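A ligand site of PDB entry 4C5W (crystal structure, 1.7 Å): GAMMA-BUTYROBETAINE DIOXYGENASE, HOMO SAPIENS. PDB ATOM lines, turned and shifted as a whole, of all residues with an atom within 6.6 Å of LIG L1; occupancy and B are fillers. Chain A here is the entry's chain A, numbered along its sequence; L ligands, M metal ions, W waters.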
ATOM      1  N   THR A 175     -13.122  32.881   3.115  1.00  0.00           N
ATOM      2  CA  THR A 175     -13.968  31.883   2.431  1.00  0.00           C
ATOM      3  C   THR A 175     -13.694  30.522   3.060  1.00  0.00           C
ATOM      4  O   THR A 175     -12.838  30.383   3.934  1.00  0.00           O
ATOM      5  CB  THR A 175     -13.691  31.795   0.913  1.00  0.00           C
ATOM      6  OG1 THR A 175     -12.410  31.184   0.681  1.00  0.00           O
ATOM      7  CG2 THR A 175     -13.730  33.169   0.254  1.00  0.00           C
ATOM      8  N   TYR A 177     -12.018  28.197   1.983  1.00  0.00           N
ATOM      9  CA  TYR A 177     -10.641  27.745   1.754  1.00  0.00           C
ATOM     10  C   TYR A 177      -9.640  28.455   2.667  1.00  0.00           C
ATOM     11  O   TYR A 177      -8.437  28.255   2.537  1.00  0.00           O
ATOM     12  CB  TYR A 177     -10.259  27.925   0.278  1.00  0.00           C
ATOM     13  CG  TYR A 177     -10.972  26.933  -0.612  1.00  0.00           C
ATOM     14  CD1 TYR A 177     -10.487  25.634  -0.770  1.00  0.00           C
ATOM     15  CD2 TYR A 177     -12.131  27.290  -1.298  1.00  0.00           C
ATOM     16  CE1 TYR A 177     -11.157  24.706  -1.573  1.00  0.00           C
ATOM     17  CE2 TYR A 177     -12.811  26.389  -2.099  1.00  0.00           C
ATOM     18  CZ  TYR A 177     -12.298  25.076  -2.218  1.00  0.00           C
ATOM     19  OH  TYR A 177     -12.946  24.148  -2.999  1.00  0.00           O
ATOM     20  N   TRP A 181      -4.672  30.877   1.355  1.00  0.00           N
ATOM     21  CA  TRP A 181      -4.682  29.495   0.946  1.00  0.00           C
ATOM     22  C   TRP A 181      -3.463  29.185   0.099  1.00  0.00           C
ATOM     23  O   TRP A 181      -2.857  30.103  -0.502  1.00  0.00           O
ATOM     24  CB  TRP A 181      -5.980  29.097   0.237  1.00  0.00           C
ATOM     25  CG  TRP A 181      -6.672  30.213  -0.455  1.00  0.00           C
ATOM     26  CD1 TRP A 181      -7.693  30.966   0.040  1.00  0.00           C
ATOM     27  CD2 TRP A 181      -6.359  30.750  -1.745  1.00  0.00           C
ATOM     28  NE1 TRP A 181      -8.053  31.921  -0.858  1.00  0.00           N
ATOM     29  CE2 TRP A 181      -7.258  31.824  -1.968  1.00  0.00           C
ATOM     30  CE3 TRP A 181      -5.438  30.408  -2.749  1.00  0.00           C
ATOM     31  CZ2 TRP A 181      -7.240  32.565  -3.145  1.00  0.00           C
ATOM     32  CZ3 TRP A 181      -5.428  31.129  -3.903  1.00  0.00           C
ATOM     33  CH2 TRP A 181      -6.341  32.203  -4.109  1.00  0.00           C
ATOM     34  N   VAL A 183      -1.700  27.280  -2.946  1.00  0.00           N
ATOM     35  CA  VAL A 183      -1.836  26.641  -4.242  1.00  0.00           C
ATOM     36  C   VAL A 183      -0.605  25.771  -4.438  1.00  0.00           C
ATOM     37  O   VAL A 183       0.475  26.256  -4.718  1.00  0.00           O
ATOM     38  CB  VAL A 183      -1.993  27.647  -5.394  1.00  0.00           C
ATOM     39  CG1 VAL A 183      -2.257  26.910  -6.678  1.00  0.00           C
ATOM     40  CG2 VAL A 183      -3.107  28.647  -5.069  1.00  0.00           C
ATOM     41  N   ASN A 190      -8.885  18.769  -2.766  1.00  0.00           N
ATOM     42  CA  ASN A 190     -10.298  19.116  -2.684  1.00  0.00           C
ATOM     43  C   ASN A 190     -10.716  20.120  -3.757  1.00  0.00           C
ATOM     44  O   ASN A 190     -11.882  20.573  -3.802  1.00  0.00           O
ATOM     45  CB  ASN A 190     -10.639  19.636  -1.289  1.00  0.00           C
ATOM     46  CG  ASN A 190      -9.960  20.968  -0.948  1.00  0.00           C
ATOM     47  OD1 ASN A 190      -9.317  21.617  -1.788  1.00  0.00           O
ATOM     48  ND2 ASN A 190     -10.150  21.397   0.281  1.00  0.00           N
ATOM     49  N   ASN A 191      -9.786  20.445  -4.657  1.00  0.00           N
ATOM     50  CA  ASN A 191     -10.012  21.431  -5.703  1.00  0.00           C
ATOM     51  C   ASN A 191      -9.004  21.184  -6.822  1.00  0.00           C
ATOM     52  O   ASN A 191      -7.864  20.866  -6.539  1.00  0.00           O
ATOM     53  CB  ASN A 191      -9.840  22.836  -5.102  1.00  0.00           C
ATOM     54  CG  ASN A 191     -10.378  23.950  -6.009  1.00  0.00           C
ATOM     55  OD1 ASN A 191      -9.763  24.308  -7.006  1.00  0.00           O
ATOM     56  ND2 ASN A 191     -11.528  24.492  -5.657  1.00  0.00           N
ATOM     57  N   VAL A 192      -9.397  21.378  -8.083  1.00  0.00           N
ATOM     58  CA  VAL A 192      -8.517  21.141  -9.226  1.00  0.00           C
ATOM     59  C   VAL A 192      -7.301  22.073  -9.184  1.00  0.00           C
ATOM     60  O   VAL A 192      -6.241  21.758  -9.736  1.00  0.00           O
ATOM     61  CB  VAL A 192      -9.282  21.306 -10.560  1.00  0.00           C
ATOM     62  CG1 VAL A 192      -8.379  21.097 -11.766  1.00  0.00           C
ATOM     63  CG2 VAL A 192     -10.429  20.320 -10.635  1.00  0.00           C
ATOM     64  N   ALA A 193      -7.463  23.227  -8.547  1.00  0.00           N
ATOM     65  CA  ALA A 193      -6.329  24.140  -8.365  1.00  0.00           C
ATOM     66  C   ALA A 193      -5.143  23.508  -7.617  1.00  0.00           C
ATOM     67  O   ALA A 193      -3.968  23.801  -7.880  1.00  0.00           O
ATOM     68  CB  ALA A 193      -6.781  25.396  -7.643  1.00  0.00           C
ATOM     69  N   TYR A 194      -5.468  22.607  -6.702  1.00  0.00           N
ATOM     70  CA  TYR A 194      -4.468  21.985  -5.843  1.00  0.00           C
ATOM     71  C   TYR A 194      -3.935  20.664  -6.449  1.00  0.00           C
ATOM     72  O   TYR A 194      -3.732  19.674  -5.761  1.00  0.00           O
ATOM     73  CB  TYR A 194      -5.078  21.744  -4.483  1.00  0.00           C
ATOM     74  CG  TYR A 194      -5.566  22.992  -3.743  1.00  0.00           C
ATOM     75  CD1 TYR A 194      -4.993  24.255  -3.969  1.00  0.00           C
ATOM     76  CD2 TYR A 194      -6.546  22.886  -2.774  1.00  0.00           C
ATOM     77  CE1 TYR A 194      -5.422  25.376  -3.266  1.00  0.00           C
ATOM     78  CE2 TYR A 194      -6.997  24.007  -2.076  1.00  0.00           C
ATOM     79  CZ  TYR A 194      -6.415  25.244  -2.320  1.00  0.00           C
ATOM     80  OH  TYR A 194      -6.826  26.342  -1.630  1.00  0.00           O
ATOM     81  N   HIS A 202     -10.618  30.866 -16.128  1.00  0.00           N
ATOM     82  CA  HIS A 202     -11.740  30.891 -15.222  1.00  0.00           C
ATOM     83  C   HIS A 202     -11.678  32.136 -14.353  1.00  0.00           C
ATOM     84  O   HIS A 202     -10.630  32.776 -14.255  1.00  0.00           O
ATOM     85  CB  HIS A 202     -11.667  29.667 -14.291  1.00  0.00           C
ATOM     86  CG  HIS A 202     -10.471  29.655 -13.401  1.00  0.00           C
ATOM     87  ND1 HIS A 202      -9.217  29.312 -13.851  1.00  0.00           N
ATOM     88  CD2 HIS A 202     -10.339  29.910 -12.070  1.00  0.00           C
ATOM     89  CE1 HIS A 202      -8.354  29.382 -12.840  1.00  0.00           C
ATOM     90  NE2 HIS A 202      -9.018  29.746 -11.757  1.00  0.00           N
ATOM     91  N   THR A 203     -12.816  32.430 -13.718  1.00  0.00           N
ATOM     92  CA  THR A 203     -12.900  33.326 -12.564  1.00  0.00           C
ATOM     93  C   THR A 203     -12.930  32.439 -11.336  1.00  0.00           C
ATOM     94  O   THR A 203     -13.380  31.291 -11.446  1.00  0.00           O
ATOM     95  CB  THR A 203     -14.168  34.219 -12.615  1.00  0.00           C
ATOM     96  OG1 THR A 203     -15.338  33.405 -12.653  1.00  0.00           O
ATOM     97  CG2 THR A 203     -14.171  35.078 -13.854  1.00  0.00           C
ATOM     98  N   ASP A 204     -12.464  32.938 -10.198  1.00  0.00           N
ATOM     99  CA  ASP A 204     -12.512  32.174  -8.970  1.00  0.00           C
ATOM    100  C   ASP A 204     -13.863  32.311  -8.282  1.00  0.00           C
ATOM    101  O   ASP A 204     -14.453  33.397  -8.193  1.00  0.00           O
ATOM    102  CB  ASP A 204     -11.421  32.595  -7.986  1.00  0.00           C
ATOM    103  CG  ASP A 204     -10.107  31.849  -8.180  1.00  0.00           C
ATOM    104  OD1 ASP A 204      -9.778  31.453  -9.315  1.00  0.00           O
ATOM    105  OD2 ASP A 204      -9.355  31.646  -7.183  1.00  0.00           O
ATOM    106  N   TYR A 205     -14.325  31.181  -7.760  1.00  0.00           N
ATOM    107  CA  TYR A 205     -15.421  31.122  -6.813  1.00  0.00           C
ATOM    108  C   TYR A 205     -16.799  31.542  -7.314  1.00  0.00           C
ATOM    109  O   TYR A 205     -17.577  32.108  -6.547  1.00  0.00           O
ATOM    110  CB  TYR A 205     -15.036  31.844  -5.493  1.00  0.00           C
ATOM    111  CG  TYR A 205     -15.033  30.940  -4.250  1.00  0.00           C
ATOM    112  CD1 TYR A 205     -16.009  29.960  -4.049  1.00  0.00           C
ATOM    113  CD2 TYR A 205     -14.077  31.108  -3.256  1.00  0.00           C
ATOM    114  CE1 TYR A 205     -16.017  29.156  -2.911  1.00  0.00           C
ATOM    115  CE2 TYR A 205     -14.074  30.332  -2.128  1.00  0.00           C
ATOM    116  CZ  TYR A 205     -15.043  29.364  -1.944  1.00  0.00           C
ATOM    117  OH  TYR A 205     -15.051  28.597  -0.787  1.00  0.00           O
ATOM    118  N   PRO A 206     -17.156  31.193  -8.571  1.00  0.00           N
ATOM    119  CA  PRO A 206     -18.539  31.399  -8.977  1.00  0.00           C
ATOM    120  C   PRO A 206     -19.533  30.550  -8.173  1.00  0.00           C
ATOM    121  O   PRO A 206     -20.717  30.792  -8.233  1.00  0.00           O
ATOM    122  CB  PRO A 206     -18.559  31.022 -10.457  1.00  0.00           C
ATOM    123  CG  PRO A 206     -17.367  30.120 -10.635  1.00  0.00           C
ATOM    124  CD  PRO A 206     -16.345  30.606  -9.658  1.00  0.00           C
ATOM    125  N   ALA A 207     -19.041  29.566  -7.427  1.00  0.00           N
ATOM    126  CA  ALA A 207     -19.926  28.800  -6.514  1.00  0.00           C
ATOM    127  C   ALA A 207     -20.503  29.662  -5.389  1.00  0.00           C
ATOM    128  O   ALA A 207     -21.460  29.263  -4.717  1.00  0.00           O
ATOM    129  CB  ALA A 207     -19.165  27.605  -5.931  1.00  0.00           C
ATOM    130  N   GLN A 215      -8.437  39.333  -6.369  1.00  0.00           N
ATOM    131  CA  GLN A 215      -7.635  38.189  -5.994  1.00  0.00           C
ATOM    132  C   GLN A 215      -6.149  38.592  -5.888  1.00  0.00           C
ATOM    133  O   GLN A 215      -5.637  39.361  -6.677  1.00  0.00           O
ATOM    134  CB  GLN A 215      -7.812  37.084  -7.037  1.00  0.00           C
ATOM    135  CG  GLN A 215      -6.986  35.833  -6.749  1.00  0.00           C
ATOM    136  CD  GLN A 215      -7.397  34.620  -7.557  1.00  0.00           C
ATOM    137  OE1 GLN A 215      -6.627  33.654  -7.688  1.00  0.00           O
ATOM    138  NE2 GLN A 215      -8.589  34.658  -8.094  1.00  0.00           N
ATOM    139  N   LEU A 217      -2.314  36.732  -5.597  1.00  0.00           N
ATOM    140  CA  LEU A 217      -1.532  35.495  -5.718  1.00  0.00           C
ATOM    141  C   LEU A 217      -0.050  35.828  -5.626  1.00  0.00           C
ATOM    142  O   LEU A 217       0.472  36.572  -6.434  1.00  0.00           O
ATOM    143  CB  LEU A 217      -1.780  34.791  -7.058  1.00  0.00           C
ATOM    144  CG  LEU A 217      -3.028  33.960  -7.337  1.00  0.00           C
ATOM    145  CD1 LEU A 217      -2.992  33.413  -8.775  1.00  0.00           C
ATOM    146  CD2 LEU A 217      -3.088  32.840  -6.344  1.00  0.00           C
ATOM    147  N   ASP A 261     -19.677  23.338  -5.040  1.00  0.00           N
ATOM    148  CA  ASP A 261     -18.413  23.025  -4.396  1.00  0.00           C
ATOM    149  C   ASP A 261     -18.737  22.306  -3.092  1.00  0.00           C
ATOM    150  O   ASP A 261     -19.443  22.850  -2.237  1.00  0.00           O
ATOM    151  CB  ASP A 261     -17.602  24.299  -4.121  1.00  0.00           C
ATOM    152  CG  ASP A 261     -16.128  24.043  -3.923  1.00  0.00           C
ATOM    153  OD1 ASP A 261     -15.623  22.948  -4.298  1.00  0.00           O
ATOM    154  OD2 ASP A 261     -15.436  24.967  -3.434  1.00  0.00           O
ATOM    155  N   ASN A 292     -16.205  29.144 -13.962  1.00  0.00           N
ATOM    156  CA  ASN A 292     -15.123  28.224 -13.675  1.00  0.00           C
ATOM    157  C   ASN A 292     -15.589  26.823 -14.119  1.00  0.00           C
ATOM    158  O   ASN A 292     -16.590  26.317 -13.601  1.00  0.00           O
ATOM    159  CB  ASN A 292     -14.740  28.242 -12.202  1.00  0.00           C
ATOM    160  CG  ASN A 292     -13.547  27.340 -11.866  1.00  0.00           C
ATOM    161  OD1 ASN A 292     -13.109  26.511 -12.672  1.00  0.00           O
ATOM    162  ND2 ASN A 292     -13.029  27.490 -10.682  1.00  0.00           N
ATOM    163  N   ALA A 294     -14.389  23.988 -13.801  1.00  0.00           N
ATOM    164  CA  ALA A 294     -14.255  22.922 -12.801  1.00  0.00           C
ATOM    165  C   ALA A 294     -15.437  22.813 -11.853  1.00  0.00           C
ATOM    166  O   ALA A 294     -15.862  21.694 -11.511  1.00  0.00           O
ATOM    167  CB  ALA A 294     -12.946  23.085 -12.046  1.00  0.00           C
ATOM    168  N   THR A 295     -15.983  23.959 -11.445  1.00  0.00           N
ATOM    169  CA  THR A 295     -17.057  23.990 -10.449  1.00  0.00           C
ATOM    170  C   THR A 295     -18.446  24.158 -11.042  1.00  0.00           C
ATOM    171  O   THR A 295     -19.439  24.148 -10.333  1.00  0.00           O
ATOM    172  CB  THR A 295     -16.810  25.077  -9.403  1.00  0.00           C
ATOM    173  OG1 THR A 295     -16.794  26.371 -10.028  1.00  0.00           O
ATOM    174  CG2 THR A 295     -15.481  24.846  -8.677  1.00  0.00           C
ATOM    175  N   HIS A 347      -8.358  33.975 -15.600  1.00  0.00           N
ATOM    176  CA  HIS A 347      -6.953  33.603 -15.445  1.00  0.00           C
ATOM    177  C   HIS A 347      -6.801  32.115 -15.564  1.00  0.00           C
ATOM    178  O   HIS A 347      -7.777  31.352 -15.417  1.00  0.00           O
ATOM    179  CB  HIS A 347      -6.389  34.119 -14.096  1.00  0.00           C
ATOM    180  CG  HIS A 347      -7.067  33.555 -12.875  1.00  0.00           C
ATOM    181  ND1 HIS A 347      -8.294  33.986 -12.450  1.00  0.00           N
ATOM    182  CD2 HIS A 347      -6.673  32.592 -12.002  1.00  0.00           C
ATOM    183  CE1 HIS A 347      -8.633  33.327 -11.351  1.00  0.00           C
ATOM    184  NE2 HIS A 347      -7.683  32.447 -11.080  1.00  0.00           N
ATOM    185  N   TYR A 366      -8.298  36.731  -1.089  1.00  0.00           N
ATOM    186  CA  TYR A 366      -9.312  37.496  -1.768  1.00  0.00           C
ATOM    187  C   TYR A 366      -9.608  38.772  -0.988  1.00  0.00           C
ATOM    188  O   TYR A 366      -9.422  38.841   0.234  1.00  0.00           O
ATOM    189  CB  TYR A 366     -10.592  36.678  -1.831  1.00  0.00           C
ATOM    190  CG  TYR A 366     -10.504  35.405  -2.643  1.00  0.00           C
ATOM    191  CD1 TYR A 366     -10.146  35.430  -3.992  1.00  0.00           C
ATOM    192  CD2 TYR A 366     -10.869  34.189  -2.071  1.00  0.00           C
ATOM    193  CE1 TYR A 366     -10.098  34.259  -4.729  1.00  0.00           C
ATOM    194  CE2 TYR A 366     -10.839  33.041  -2.812  1.00  0.00           C
ATOM    195  CZ  TYR A 366     -10.450  33.069  -4.133  1.00  0.00           C
ATOM    196  OH  TYR A 366     -10.443  31.857  -4.847  1.00  0.00           O
HETATM  197  N1  LIG L   1      -9.091  28.210  -4.588  1.00  0.00           N
HETATM  198  C1  LIG L   1      -9.174  26.749  -4.287  1.00  0.00           C
HETATM  199  O1  LIG L   1     -13.689  28.440  -8.040  1.00  0.00           O
HETATM  200  C2  LIG L   1     -12.710  27.911  -7.465  1.00  0.00           C
HETATM  201  O2  LIG L   1     -12.788  26.863  -6.787  1.00  0.00           O
HETATM  202  C3  LIG L   1     -11.381  28.577  -7.718  1.00  0.00           C
HETATM  203  C4  LIG L   1     -10.234  28.594  -5.470  1.00  0.00           C
HETATM  204  C5  LIG L   1      -9.198  29.015  -3.339  1.00  0.00           C
HETATM  205  C6  LIG L   1      -7.783  28.493  -5.192  1.00  0.00           C
HETATM  206  C7  LIG L   1     -10.213  28.031  -6.879  1.00  0.00           C
HETATM  207  C1  LG2 L   2      -6.368  29.058  -8.651  1.00  0.00           C
HETATM  208  C2  LG2 L   2      -5.462  29.520  -9.694  1.00  0.00           C
HETATM  209  C3  LG2 L   2      -3.287  29.828 -10.677  1.00  0.00           C
HETATM  210  C4  LG2 L   2      -1.909  29.198 -10.608  1.00  0.00           C
HETATM  211  O1  LG2 L   2      -5.875  28.420  -7.703  1.00  0.00           O
HETATM  212  O2  LG2 L   2      -7.602  29.358  -8.740  1.00  0.00           O
HETATM  213  O3  LG2 L   2      -5.951  30.128 -10.614  1.00  0.00           O
HETATM  214  O4  LG2 L   2      -1.030  29.785 -11.245  1.00  0.00           O
HETATM  215  N1  LG2 L   2      -4.154  29.298  -9.638  1.00  0.00           N
HETATM  216  O5  LG2 L   2      -1.719  28.128  -9.934  1.00  0.00           O
HETATM  217 ZN    ZN M   1      -8.092  30.657 -10.144  1.00  0.00          ZN
HETATM  218  O   HOH W   1     -11.344  25.192  -9.236  1.00  0.00           O
HETATM  219  O   HOH W   2     -16.430  27.940  -7.600  1.00  0.00           O
HETATM  220  O   HOH W   3     -15.354  26.690  -5.557  1.00  0.00           O
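O1 of LIG L1 lies within hydrogen-bond range of N of Tyr 205. An oxygen (O1) of LIG L1 is in hydrogen-bond range of the side-chain amide nitrogen (ND2) of Asn 292 (2.9 Å). O2 of LIG L1 is in hydrogen-bond range of ND2 of Asn 191 (2.9 Å).
The side-chain amide oxygen (OD1) of Asn 292 is in hydrogen-bond range of the backbone NH (N) of Ala 294. The side-chain amide nitrogen of Asn 191 lies within hydrogen-bond range of the side-chain hydroxyl of Tyr 177 (3.0 Å). The side-chain amide oxygen (OD1) of Asn 191 lies within hydrogen-bond range of the backbone NH (N) of Ala 193 (3.0 Å). The side-chain hydroxyl (OH) of Tyr 366 lies within hydrogen-bond range of the side-chain carboxylate (OD2) of Asp 204, 2.6 Å away. The side-chain carboxylate (OD2) of Asp 204 lies close to the side-chain amide nitrogen (NE2) of Gln 215, 3.2 Å away. OD2 of Asp 261 sits at hydrogen-bond distance from OH of Tyr 177 (2.7 Å). The backbone NH (N) of Tyr 177 sits close to the side-chain hydroxyl (OG1) of Thr 175 (3.3 Å).
CG of Tyr 177 touches C5 of LIG L1 (3.9 Å). CE2 of Trp 181 touches C5 of LIG L1, 3.7 Å away. Tyr 194 touches LIG L1. Asp 204 touches LIG L1 (CG to C3, 3.5 Å). Pro 206 touches LIG L1 (CD to O1, 3.8 Å). Thr 295 touches LIG L1 (CG2 to O2, 3.9 Å). Tyr 366 touches LIG L1. Ten residues have an atom within 4 Å of LIG L1: Tyr 177, Trp 181, Asn 191, Tyr 194, Asp 204, Tyr 205, Pro 206, Asn 292, Thr 295 and Tyr 366. Along chain A the residues within 4 Å of LIG L1 span positions 177 to 366. The nearest printed residue that does not touch LIG L1 is Ala 193 (4.1 Å).
Water W2 lies within hydrogen-bond range of an oxygen (O1) of LIG L1 (2.8 Å), the side-chain hydroxyl (OG1) of Thr 295 (2.9 Å) and the backbone NH (N) of Ala 207 (3.1 Å). Water W3 bridges OD2 of Asp 261 (2.7 Å) and O2 of LIG L1 (2.9 Å). Water W1 lies within hydrogen-bond range of OD1 of Asn 191, ND2 of Asn 292 and O2 of LIG L1.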
